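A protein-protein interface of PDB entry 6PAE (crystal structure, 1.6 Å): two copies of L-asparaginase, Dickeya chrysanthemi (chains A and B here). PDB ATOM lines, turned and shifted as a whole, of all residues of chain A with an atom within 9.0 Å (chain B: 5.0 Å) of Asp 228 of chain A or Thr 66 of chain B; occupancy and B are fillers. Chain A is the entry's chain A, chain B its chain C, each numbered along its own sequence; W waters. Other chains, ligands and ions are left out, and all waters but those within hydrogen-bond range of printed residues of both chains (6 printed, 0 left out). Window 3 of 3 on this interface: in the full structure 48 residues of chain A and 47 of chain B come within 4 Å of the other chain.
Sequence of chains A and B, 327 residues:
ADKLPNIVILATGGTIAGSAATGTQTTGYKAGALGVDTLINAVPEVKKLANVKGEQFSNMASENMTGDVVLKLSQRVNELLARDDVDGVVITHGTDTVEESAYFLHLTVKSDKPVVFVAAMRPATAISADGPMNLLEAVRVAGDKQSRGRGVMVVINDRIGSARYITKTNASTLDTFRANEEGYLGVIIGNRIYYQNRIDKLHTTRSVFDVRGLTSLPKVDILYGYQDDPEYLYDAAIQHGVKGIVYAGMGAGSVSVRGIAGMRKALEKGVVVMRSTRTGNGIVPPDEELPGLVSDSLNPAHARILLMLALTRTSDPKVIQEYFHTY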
ATOM      1  N   TYR A 224       9.141 -12.594 -11.330  1.00  0.00           N
ATOM      2  CA  TYR A 224       9.582 -12.536  -9.932  1.00  0.00           C
ATOM      3  C   TYR A 224       9.844 -13.935  -9.359  1.00  0.00           C
ATOM      4  O   TYR A 224       9.192 -14.896  -9.793  1.00  0.00           O
ATOM      5  CB  TYR A 224       8.527 -11.785  -9.121  1.00  0.00           C
ATOM      6  CG  TYR A 224       9.037 -11.034  -7.901  1.00  0.00           C
ATOM      7  CD1 TYR A 224       9.740  -9.870  -8.090  1.00  0.00           C
ATOM      8  CD2 TYR A 224       8.705 -11.407  -6.612  1.00  0.00           C
ATOM      9  CE1 TYR A 224      10.143  -9.136  -7.024  1.00  0.00           C
ATOM     10  CE2 TYR A 224       9.127 -10.677  -5.533  1.00  0.00           C
ATOM     11  CZ  TYR A 224       9.804  -9.547  -5.743  1.00  0.00           C
ATOM     12  OH  TYR A 224      10.240  -8.739  -4.668  1.00  0.00           O
ATOM     13  N   GLY A 225      10.777 -14.030  -8.405  1.00  0.00           N
ATOM     14  CA  GLY A 225      11.014 -15.233  -7.633  1.00  0.00           C
ATOM     15  C   GLY A 225      10.515 -15.065  -6.172  1.00  0.00           C
ATOM     16  O   GLY A 225      10.741 -14.038  -5.508  1.00  0.00           O
ATOM     17  N   TYR A 226       9.864 -16.120  -5.663  1.00  0.00           N
ATOM     18  CA  TYR A 226       9.143 -16.158  -4.415  1.00  0.00           C
ATOM     19  C   TYR A 226       8.654 -17.590  -4.160  1.00  0.00           C
ATOM     20  O   TYR A 226       8.613 -18.405  -5.097  1.00  0.00           O
ATOM     21  CB  TYR A 226       7.983 -15.215  -4.381  1.00  0.00           C
ATOM     22  CG  TYR A 226       6.985 -15.375  -5.486  1.00  0.00           C
ATOM     23  CD1 TYR A 226       7.262 -14.885  -6.731  1.00  0.00           C
ATOM     24  CD2 TYR A 226       5.731 -15.897  -5.244  1.00  0.00           C
ATOM     25  CE1 TYR A 226       6.319 -14.937  -7.720  1.00  0.00           C
ATOM     26  CE2 TYR A 226       4.774 -16.019  -6.243  1.00  0.00           C
ATOM     27  CZ  TYR A 226       5.069 -15.512  -7.478  1.00  0.00           C
ATOM     28  OH  TYR A 226       4.218 -15.507  -8.570  1.00  0.00           O
ATOM     29  N   GLN A 227       8.316 -17.848  -2.906  1.00  0.00           N
ATOM     30  CA  GLN A 227       7.796 -19.178  -2.570  1.00  0.00           C
ATOM     31  C   GLN A 227       6.578 -19.430  -3.464  1.00  0.00           C
ATOM     32  O   GLN A 227       5.743 -18.559  -3.607  1.00  0.00           O
ATOM     33  CB  GLN A 227       7.396 -19.279  -1.116  1.00  0.00           C
ATOM     34  CG  GLN A 227       8.575 -19.190  -0.175  1.00  0.00           C
ATOM     35  CD  GLN A 227       8.165 -19.346   1.278  1.00  0.00           C
ATOM     36  OE1 GLN A 227       6.990 -19.349   1.593  1.00  0.00           O
ATOM     37  NE2 GLN A 227       9.134 -19.380   2.183  1.00  0.00           N
ATOM     38  N   ASP A 228       6.483 -20.638  -3.994  1.00  0.00           N
ATOM     39  CA  ASP A 228       5.313 -21.097  -4.833  1.00  0.00           C
ATOM     40  C   ASP A 228       5.244 -20.380  -6.169  1.00  0.00           C
ATOM     41  O   ASP A 228       4.197 -20.448  -6.845  1.00  0.00           O
ATOM     42  CB  ASP A 228       3.973 -20.973  -4.083  1.00  0.00           C
ATOM     43  CG  ASP A 228       3.959 -21.702  -2.785  1.00  0.00           C
ATOM     44  OD1 ASP A 228       4.108 -22.962  -2.791  1.00  0.00           O
ATOM     45  OD2 ASP A 228       3.876 -21.032  -1.734  1.00  0.00           O
ATOM     46  N   ASP A 229       6.369 -19.823  -6.638  1.00  0.00           N
ATOM     47  CA  ASP A 229       6.354 -19.147  -7.932  1.00  0.00           C
ATOM     48  C   ASP A 229       5.896 -20.106  -9.045  1.00  0.00           C
ATOM     49  O   ASP A 229       6.375 -21.239  -9.136  1.00  0.00           O
ATOM     50  CB  ASP A 229       7.707 -18.466  -8.266  1.00  0.00           C
ATOM     51  CG  ASP A 229       8.894 -19.432  -8.411  1.00  0.00           C
ATOM     52  OD1 ASP A 229       8.959 -20.444  -7.753  1.00  0.00           O
ATOM     53  OD2 ASP A 229       9.801 -19.155  -9.255  1.00  0.00           O
ATOM     54  N   PRO A 230       5.082 -19.587  -9.961  1.00  0.00           N
ATOM     55  CA  PRO A 230       4.429 -20.554 -10.898  1.00  0.00           C
ATOM     56  C   PRO A 230       5.209 -20.722 -12.210  1.00  0.00           C
ATOM     57  O   PRO A 230       5.767 -19.783 -12.794  1.00  0.00           O
ATOM     58  CB  PRO A 230       3.079 -19.872 -11.144  1.00  0.00           C
ATOM     59  CG  PRO A 230       3.415 -18.438 -11.138  1.00  0.00           C
ATOM     60  CD  PRO A 230       4.351 -18.325  -9.940  1.00  0.00           C
ATOM     61  N   GLU A 231       5.314 -21.991 -12.637  1.00  0.00           N
ATOM     62  CA  GLU A 231       5.926 -22.298 -13.917  1.00  0.00           C
ATOM     63  C   GLU A 231       5.157 -21.659 -15.094  1.00  0.00           C
ATOM     64  O   GLU A 231       5.774 -21.240 -16.105  1.00  0.00           O
ATOM     65  CB  GLU A 231       6.062 -23.810 -14.135  1.00  0.00           C
ATOM     66  CG  GLU A 231       6.741 -24.183 -15.448  1.00  0.00           C
ATOM     67  CD  GLU A 231       6.820 -25.678 -15.629  1.00  0.00           C
ATOM     68  OE1 GLU A 231       6.494 -26.354 -14.647  1.00  0.00           O
ATOM     69  OE2 GLU A 231       7.205 -26.156 -16.727  1.00  0.00           O
ATOM     70  N   TYR A 232       3.849 -21.546 -14.984  1.00  0.00           N
ATOM     71  CA  TYR A 232       2.995 -21.121 -16.117  1.00  0.00           C
ATOM     72  C   TYR A 232       3.297 -19.731 -16.590  1.00  0.00           C
ATOM     73  O   TYR A 232       3.066 -19.435 -17.775  1.00  0.00           O
ATOM     74  CB  TYR A 232       1.478 -21.262 -15.867  1.00  0.00           C
ATOM     75  CG  TYR A 232       0.952 -20.493 -14.702  1.00  0.00           C
ATOM     76  CD1 TYR A 232       0.674 -19.149 -14.796  1.00  0.00           C
ATOM     77  CD2 TYR A 232       0.628 -21.169 -13.544  1.00  0.00           C
ATOM     78  CE1 TYR A 232       0.152 -18.447 -13.697  1.00  0.00           C
ATOM     79  CE2 TYR A 232       0.100 -20.504 -12.473  1.00  0.00           C
ATOM     80  CZ  TYR A 232      -0.143 -19.142 -12.563  1.00  0.00           C
ATOM     81  OH  TYR A 232      -0.681 -18.533 -11.449  1.00  0.00           O
ATOM     82  N   LEU A 233       3.919 -18.869 -15.767  1.00  0.00           N
ATOM     83  CA  LEU A 233       4.262 -17.536 -16.285  1.00  0.00           C
ATOM     84  C   LEU A 233       5.430 -17.542 -17.259  1.00  0.00           C
ATOM     85  O   LEU A 233       5.479 -16.692 -18.125  1.00  0.00           O
ATOM     86  CB  LEU A 233       4.529 -16.562 -15.127  1.00  0.00           C
ATOM     87  CG  LEU A 233       3.310 -16.327 -14.250  1.00  0.00           C
ATOM     88  CD1 LEU A 233       3.772 -15.466 -13.082  1.00  0.00           C
ATOM     89  CD2 LEU A 233       2.200 -15.708 -15.058  1.00  0.00           C
ATOM     90  N   MET A 250      15.078 -15.028  -6.082  1.00  0.00           N
ATOM     91  CA  MET A 250      15.256 -15.124  -4.625  1.00  0.00           C
ATOM     92  C   MET A 250      16.731 -15.103  -4.327  1.00  0.00           C
ATOM     93  O   MET A 250      17.488 -15.785  -4.996  1.00  0.00           O
ATOM     94  CB  MET A 250      14.649 -16.506  -4.176  1.00  0.00           C
ATOM     95  CG  MET A 250      13.149 -16.497  -4.212  1.00  0.00           C
ATOM     96  SD  MET A 250      12.321 -18.084  -4.027  1.00  0.00           S
ATOM     97  CE  MET A 250      12.322 -18.785  -5.664  1.00  0.00           C
ATOM     98  N   SER A 256      13.564 -21.939  -7.862  1.00  0.00           N
ATOM     99  CA  SER A 256      12.767 -23.134  -7.468  1.00  0.00           C
ATOM    100  C   SER A 256      12.722 -24.170  -8.571  1.00  0.00           C
ATOM    101  O   SER A 256      13.057 -23.919  -9.707  1.00  0.00           O
ATOM    102  CB  SER A 256      11.335 -22.800  -7.130  1.00  0.00           C
ATOM    103  OG  SER A 256      10.639 -22.430  -8.310  1.00  0.00           O
ATOM    104  N   VAL A 257      12.254 -25.368  -8.197  1.00  0.00           N
ATOM    105  CA  VAL A 257      12.096 -26.415  -9.204  1.00  0.00           C
ATOM    106  C   VAL A 257      11.152 -25.972 -10.328  1.00  0.00           C
ATOM    107  O   VAL A 257      11.348 -26.362 -11.506  1.00  0.00           O
ATOM    108  CB  VAL A 257      11.727 -27.782  -8.603  1.00  0.00           C
ATOM    109  CG1 VAL A 257      12.881 -28.323  -7.811  1.00  0.00           C
ATOM    110  CG2 VAL A 257      10.494 -27.719  -7.734  1.00  0.00           C
ATOM    111  N   ARG A 258      10.140 -25.150 -10.006  1.00  0.00           N
ATOM    112  CA  ARG A 258       9.172 -24.669 -10.982  1.00  0.00           C
ATOM    113  C   ARG A 258       9.806 -23.670 -11.913  1.00  0.00           C
ATOM    114  O   ARG A 258       9.675 -23.697 -13.120  1.00  0.00           O
ATOM    115  CB  ARG A 258       7.955 -24.100 -10.237  1.00  0.00           C
ATOM    116  CG  ARG A 258       7.200 -25.125  -9.380  1.00  0.00           C
ATOM    117  CD  ARG A 258       6.077 -24.560  -8.502  1.00  0.00           C
ATOM    118  NE  ARG A 258       6.695 -23.512  -7.706  1.00  0.00           N
ATOM    119  CZ  ARG A 258       7.436 -23.750  -6.652  1.00  0.00           C
ATOM    120  NH1 ARG A 258       7.575 -24.965  -6.157  1.00  0.00           N
ATOM    121  NH2 ARG A 258       8.043 -22.736  -6.054  1.00  0.00           N
ATOM    122  N   GLY A 259      10.578 -22.768 -11.340  1.00  0.00           N
ATOM    123  CA  GLY A 259      11.305 -21.800 -12.157  1.00  0.00           C
ATOM    124  C   GLY A 259      12.338 -22.468 -13.060  1.00  0.00           C
ATOM    125  O   GLY A 259      12.529 -22.024 -14.188  1.00  0.00           O
ATOM    126  N   ARG A 278      15.799 -10.127  -6.587  1.00  0.00           N
ATOM    127  CA  ARG A 278      14.739  -9.278  -6.053  1.00  0.00           C
ATOM    128  C   ARG A 278      15.253  -8.418  -4.834  1.00  0.00           C
ATOM    129  O   ARG A 278      14.502  -7.568  -4.283  1.00  0.00           O
ATOM    130  CB  ARG A 278      13.555 -10.138  -5.601  1.00  0.00           C
ATOM    131  CG  ARG A 278      13.735 -10.865  -4.247  1.00  0.00           C
ATOM    132  CD  ARG A 278      12.586 -11.772  -3.945  1.00  0.00           C
ATOM    133  NE  ARG A 278      12.680 -12.177  -2.535  1.00  0.00           N
ATOM    134  CZ  ARG A 278      11.909 -13.081  -1.947  1.00  0.00           C
ATOM    135  NH1 ARG A 278      10.999 -13.658  -2.607  1.00  0.00           N
ATOM    136  NH2 ARG A 278      12.024 -13.337  -0.633  1.00  0.00           N
ATOM    137  N   ASN B  64      12.924 -23.479  -2.483  1.00  0.00           N
ATOM    138  CA  ASN B  64      11.925 -24.508  -2.695  1.00  0.00           C
ATOM    139  C   ASN B  64      10.914 -24.620  -1.606  1.00  0.00           C
ATOM    140  O   ASN B  64      10.019 -25.496  -1.673  1.00  0.00           O
ATOM    141  CB  ASN B  64      12.589 -25.866  -2.946  1.00  0.00           C
ATOM    142  CG  ASN B  64      13.067 -25.967  -4.359  1.00  0.00           C
ATOM    143  OD1 ASN B  64      12.274 -25.644  -5.280  1.00  0.00           O
ATOM    144  ND2 ASN B  64      14.354 -26.231  -4.556  1.00  0.00           N
ATOM    145  N   MET B  65      10.999 -23.776  -0.593  1.00  0.00           N
ATOM    146  CA  MET B  65      10.015 -23.738   0.460  1.00  0.00           C
ATOM    147  C   MET B  65       8.655 -23.311  -0.097  1.00  0.00           C
ATOM    148  O   MET B  65       8.549 -22.370  -0.931  1.00  0.00           O
ATOM    149  CB  MET B  65      10.506 -22.827   1.596  1.00  0.00           C
ATOM    150  CG  MET B  65       9.558 -22.756   2.760  1.00  0.00           C
ATOM    151  SD  MET B  65       9.283 -24.388   3.598  1.00  0.00           S
ATOM    152  CE  MET B  65      10.891 -24.857   3.987  1.00  0.00           C
ATOM    153  N   THR B  66       7.589 -24.007   0.271  1.00  0.00           N
ATOM    154  CA  THR B  66       6.258 -23.759  -0.262  1.00  0.00           C
ATOM    155  C   THR B  66       5.261 -23.470   0.853  1.00  0.00           C
ATOM    156  O   THR B  66       5.440 -23.945   2.003  1.00  0.00           O
ATOM    157  CB  THR B  66       5.775 -24.982  -1.036  1.00  0.00           C
ATOM    158  OG1 THR B  66       5.872 -26.167  -0.239  1.00  0.00           O
ATOM    159  CG2 THR B  66       6.583 -25.148  -2.337  1.00  0.00           C
ATOM    160  N   GLY B  67       4.234 -22.708   0.548  1.00  0.00           N
ATOM    161  CA  GLY B  67       3.179 -22.402   1.489  1.00  0.00           C
ATOM    162  C   GLY B  67       2.671 -23.572   2.272  1.00  0.00           C
ATOM    163  O   GLY B  67       2.509 -23.504   3.485  1.00  0.00           O
ATOM    164  N   ASP B  68       2.447 -24.678   1.590  1.00  0.00           N
ATOM    165  CA  ASP B  68       1.911 -25.863   2.300  1.00  0.00           C
ATOM    166  C   ASP B  68       2.839 -26.385   3.343  1.00  0.00           C
ATOM    167  O   ASP B  68       2.382 -26.789   4.402  1.00  0.00           O
ATOM    168  CB  ASP B  68       1.507 -26.987   1.353  1.00  0.00           C
ATOM    169  CG  ASP B  68       0.295 -26.635   0.480  1.00  0.00           C
ATOM    170  OD1 ASP B  68      -0.454 -25.627   0.732  1.00  0.00           O
ATOM    171  OD2 ASP B  68       0.064 -27.432  -0.483  1.00  0.00           O
ATOM    172  N   VAL B  69       4.143 -26.329   3.095  1.00  0.00           N
ATOM    173  CA  VAL B  69       5.116 -26.712   4.064  1.00  0.00           C
ATOM    174  C   VAL B  69       5.291 -25.672   5.192  1.00  0.00           C
ATOM    175  O   VAL B  69       5.413 -26.037   6.388  1.00  0.00           O
ATOM    176  CB  VAL B  69       6.457 -27.050   3.417  1.00  0.00           C
ATOM    177  CG1 VAL B  69       7.461 -27.358   4.486  1.00  0.00           C
ATOM    178  CG2 VAL B  69       6.227 -28.222   2.442  1.00  0.00           C
ATOM    179  N   VAL B  70       5.226 -24.394   4.821  1.00  0.00           N
ATOM    180  CA  VAL B  70       5.329 -23.334   5.839  1.00  0.00           C
ATOM    181  C   VAL B  70       4.146 -23.431   6.797  1.00  0.00           C
ATOM    182  O   VAL B  70       4.276 -23.255   8.009  1.00  0.00           O
ATOM    183  CB  VAL B  70       5.348 -21.949   5.180  1.00  0.00           C
ATOM    184  CG1 VAL B  70       5.370 -20.911   6.283  1.00  0.00           C
ATOM    185  CG2 VAL B  70       6.546 -21.817   4.246  1.00  0.00           C
ATOM    186  N   LEU B  71       2.979 -23.761   6.244  1.00  0.00           N
ATOM    187  CA  LEU B  71       1.823 -23.945   7.072  1.00  0.00           C
ATOM    188  C   LEU B  71       2.043 -25.061   8.070  1.00  0.00           C
ATOM    189  O   LEU B  71       1.710 -24.926   9.260  1.00  0.00           O
ATOM    190  CB  LEU B  71       0.668 -24.291   6.121  1.00  0.00           C
ATOM    191  CG  LEU B  71      -0.652 -24.732   6.651  1.00  0.00           C
ATOM    192  CD1 LEU B  71      -1.190 -23.707   7.586  1.00  0.00           C
ATOM    193  CD2 LEU B  71      -1.578 -24.927   5.419  1.00  0.00           C
ATOM    194  N   ASP B 221      -0.047 -14.709  -6.758  1.00  0.00           N
ATOM    195  CA  ASP B 221       1.165 -14.562  -7.559  1.00  0.00           C
ATOM    196  C   ASP B 221       1.618 -13.109  -7.449  1.00  0.00           C
ATOM    197  O   ASP B 221       0.808 -12.230  -7.098  1.00  0.00           O
ATOM    198  CB  ASP B 221       0.940 -15.043  -9.020  1.00  0.00           C
ATOM    199  CG  ASP B 221       0.972 -16.557  -9.120  1.00  0.00           C
ATOM    200  OD1 ASP B 221       1.698 -17.206  -8.335  1.00  0.00           O
ATOM    201  OD2 ASP B 221       0.272 -17.103  -9.970  1.00  0.00           O
ATOM    202  N   ARG B 304       2.530 -10.776  -0.145  1.00  0.00           N
ATOM    203  CA  ARG B 304       1.925 -12.016  -0.637  1.00  0.00           C
ATOM    204  C   ARG B 304       1.532 -12.870   0.560  1.00  0.00           C
ATOM    205  O   ARG B 304       0.429 -13.460   0.550  1.00  0.00           O
ATOM    206  CB  ARG B 304       2.838 -12.796  -1.543  1.00  0.00           C
ATOM    207  CG  ARG B 304       2.388 -14.210  -1.850  1.00  0.00           C
ATOM    208  CD  ARG B 304       3.231 -14.842  -2.949  1.00  0.00           C
ATOM    209  NE  ARG B 304       2.861 -16.258  -3.027  1.00  0.00           N
ATOM    210  CZ  ARG B 304       3.208 -17.179  -2.165  1.00  0.00           C
ATOM    211  NH1 ARG B 304       4.092 -16.930  -1.196  1.00  0.00           N
ATOM    212  NH2 ARG B 304       2.671 -18.413  -2.283  1.00  0.00           N
HETATM  213  O   HOH W   1      -0.201 -20.171  -8.442  1.00  0.00           O
HETATM  214  O   HOH W   2       9.345 -22.367  -3.615  1.00  0.00           O
HETATM  215  O   HOH W   3       9.580 -26.178  -4.416  1.00  0.00           O
HETATM  216  O   HOH W   4       2.149 -24.378  -1.411  1.00  0.00           O
HETATM  217  O   HOH W   5       4.490 -19.325   0.556  1.00  0.00           O
HETATM  218  O   HOH W   6       1.662 -19.098  -6.753  1.00  0.00           O
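OH of Tyr 232 of chain A sits close to OD2 of Asp 221 of chain B, 2.3 Å away. The side-chain hydroxyl of Tyr 226 of chain A is in hydrogen-bond range of the side-chain carboxylate of Asp 221 of chain B, 3.0 Å away. OD1 of Asn 64 of chain B is in hydrogen-bond range of N of Val 257 of chain A, 2.9 Å away. NH2 of Arg 304 of chain B is in salt-bridge range of OD2 of Asp 228 of chain A (2.9 Å). The backbone NH of Gly 67 of chain B lies within hydrogen-bond range of the side-chain carboxylate of Asp 228 of chain A (2.9 Å). The backbone carbonyl oxygen (O) of Gln 227 of chain A lies close to the guanidinium group (NH1) of Arg 304 of chain B, at 3.3 Å.
N of Arg 258 of chain A sits close to OG of Ser 256 of chain A, 3.2 Å away. SD of Met 250 of chain A is in hydrogen-bond range of N of Tyr 226 of chain A, 3.5 Å away. The side-chain hydroxyl (OG) of Ser 256 of chain A sits at hydrogen-bond distance from the backbone NH (N) of Gly 259 of chain A. OD1 of Asp 229 of chain A lies within salt-bridge range of NH2 of Arg 258 of chain A. The side-chain carboxylate of Asp 229 of chain A lies within hydrogen-bond range of the side-chain hydroxyl of Ser 256 of chain A.
Among the printed residues, pairs that only touch across the chains: Tyr 226 of chain A with Arg 304 of chain B, Gln 227 of chain A with Met 65 of chain B, Gln 227 of chain A with Val 70 of chain B, Asp 228 of chain A with Thr 66 of chain B, Pro 230 of chain A with Asp 221 of chain B, Ser 256 of chain A with Asn 64 of chain B and Arg 258 of chain A with Thr 66 of chain B.
Of chain B, only Thr 66 (3.2 Å), Gly 67 (2.9 Å) and Arg 304 (2.9 Å) come within 4 Å of Asp 228 of chain A. No residue of chain A comes within 4 Å of Val 69 of chain B. Printed residues of chain B within 4 Å of Val 257 of chain A: Asn 64 (2.9 Å). Of the printed residues of chain B, Arg 258 of chain A touches Thr 66. Printed residues of chain A within 4 Å of Val 70 of chain B: Gln 227 (3.7 Å). Printed residues of chain B within 4 Å of Gln 227 of chain A: Met 65, Val 70 and Arg 304. Printed residues of chain A within 4 Å of Met 65 of chain B: Gln 227. Asp 68 of chain B touches none of the printed residues of chain A. The nearest residue of chain B that does not touch Asp 228 of chain A is Met 65 of chain B (4.1 Å).
Hydrophobic or aromatic side chains of chain B that line the printed part of chain A: Met 65 and Val 70. Hydrophobic or aromatic side chains of chain A within 4 Å of the printed part of chain B: Tyr 226, Pro 230, Tyr 232 and Val 257. Among the printed residues, Asp or Glu carboxylates within 4 Å of a Lys or Arg side-chain nitrogen of the other chain: Asp 228 of chain A with Arg 304 of chain B.
No position is printed for both chains.
Water W6 bridges the side-chain carboxylate of Asp 221 of chain B (2.5 Å) and the backbone carbonyl oxygen of Asp 228 of chain A (2.9 Å). Water W5 lies within hydrogen-bond range of the side-chain amide oxygen (OE1) of Gln 227 of chain A (2.7 Å), the side-chain carboxylate (OD2) of Asp 228 of chain A (2.9 Å), the guanidinium group (NH1) of Arg 304 of chain B (3.0 Å) and the backbone NH (N) of Gly 67 of chain B (3.4 Å). Water W4 lies within hydrogen-bond range of the side-chain carboxylate (OD1) of Asp 228 of chain A, the backbone NH (N) of Asp 68 of chain B and the backbone NH (N) of Gly 67 of chain B. Water W2 lies within hydrogen-bond range of the guanidinium group (NH2) of Arg 258 of chain A (2.8 Å), the backbone carbonyl oxygen (O) of Met 65 of chain B (2.8 Å) and the backbone NH (N) of Asp 228 of chain A (3.4 Å). Water W3 bridges O of Asn 64 of chain B (2.9 Å) and NH1 of Arg 258 of chain A (2.9 Å). Water W1 lies within hydrogen-bond range of OH of Tyr 232 of chain A and OD2 of Asp 221 of chain B.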
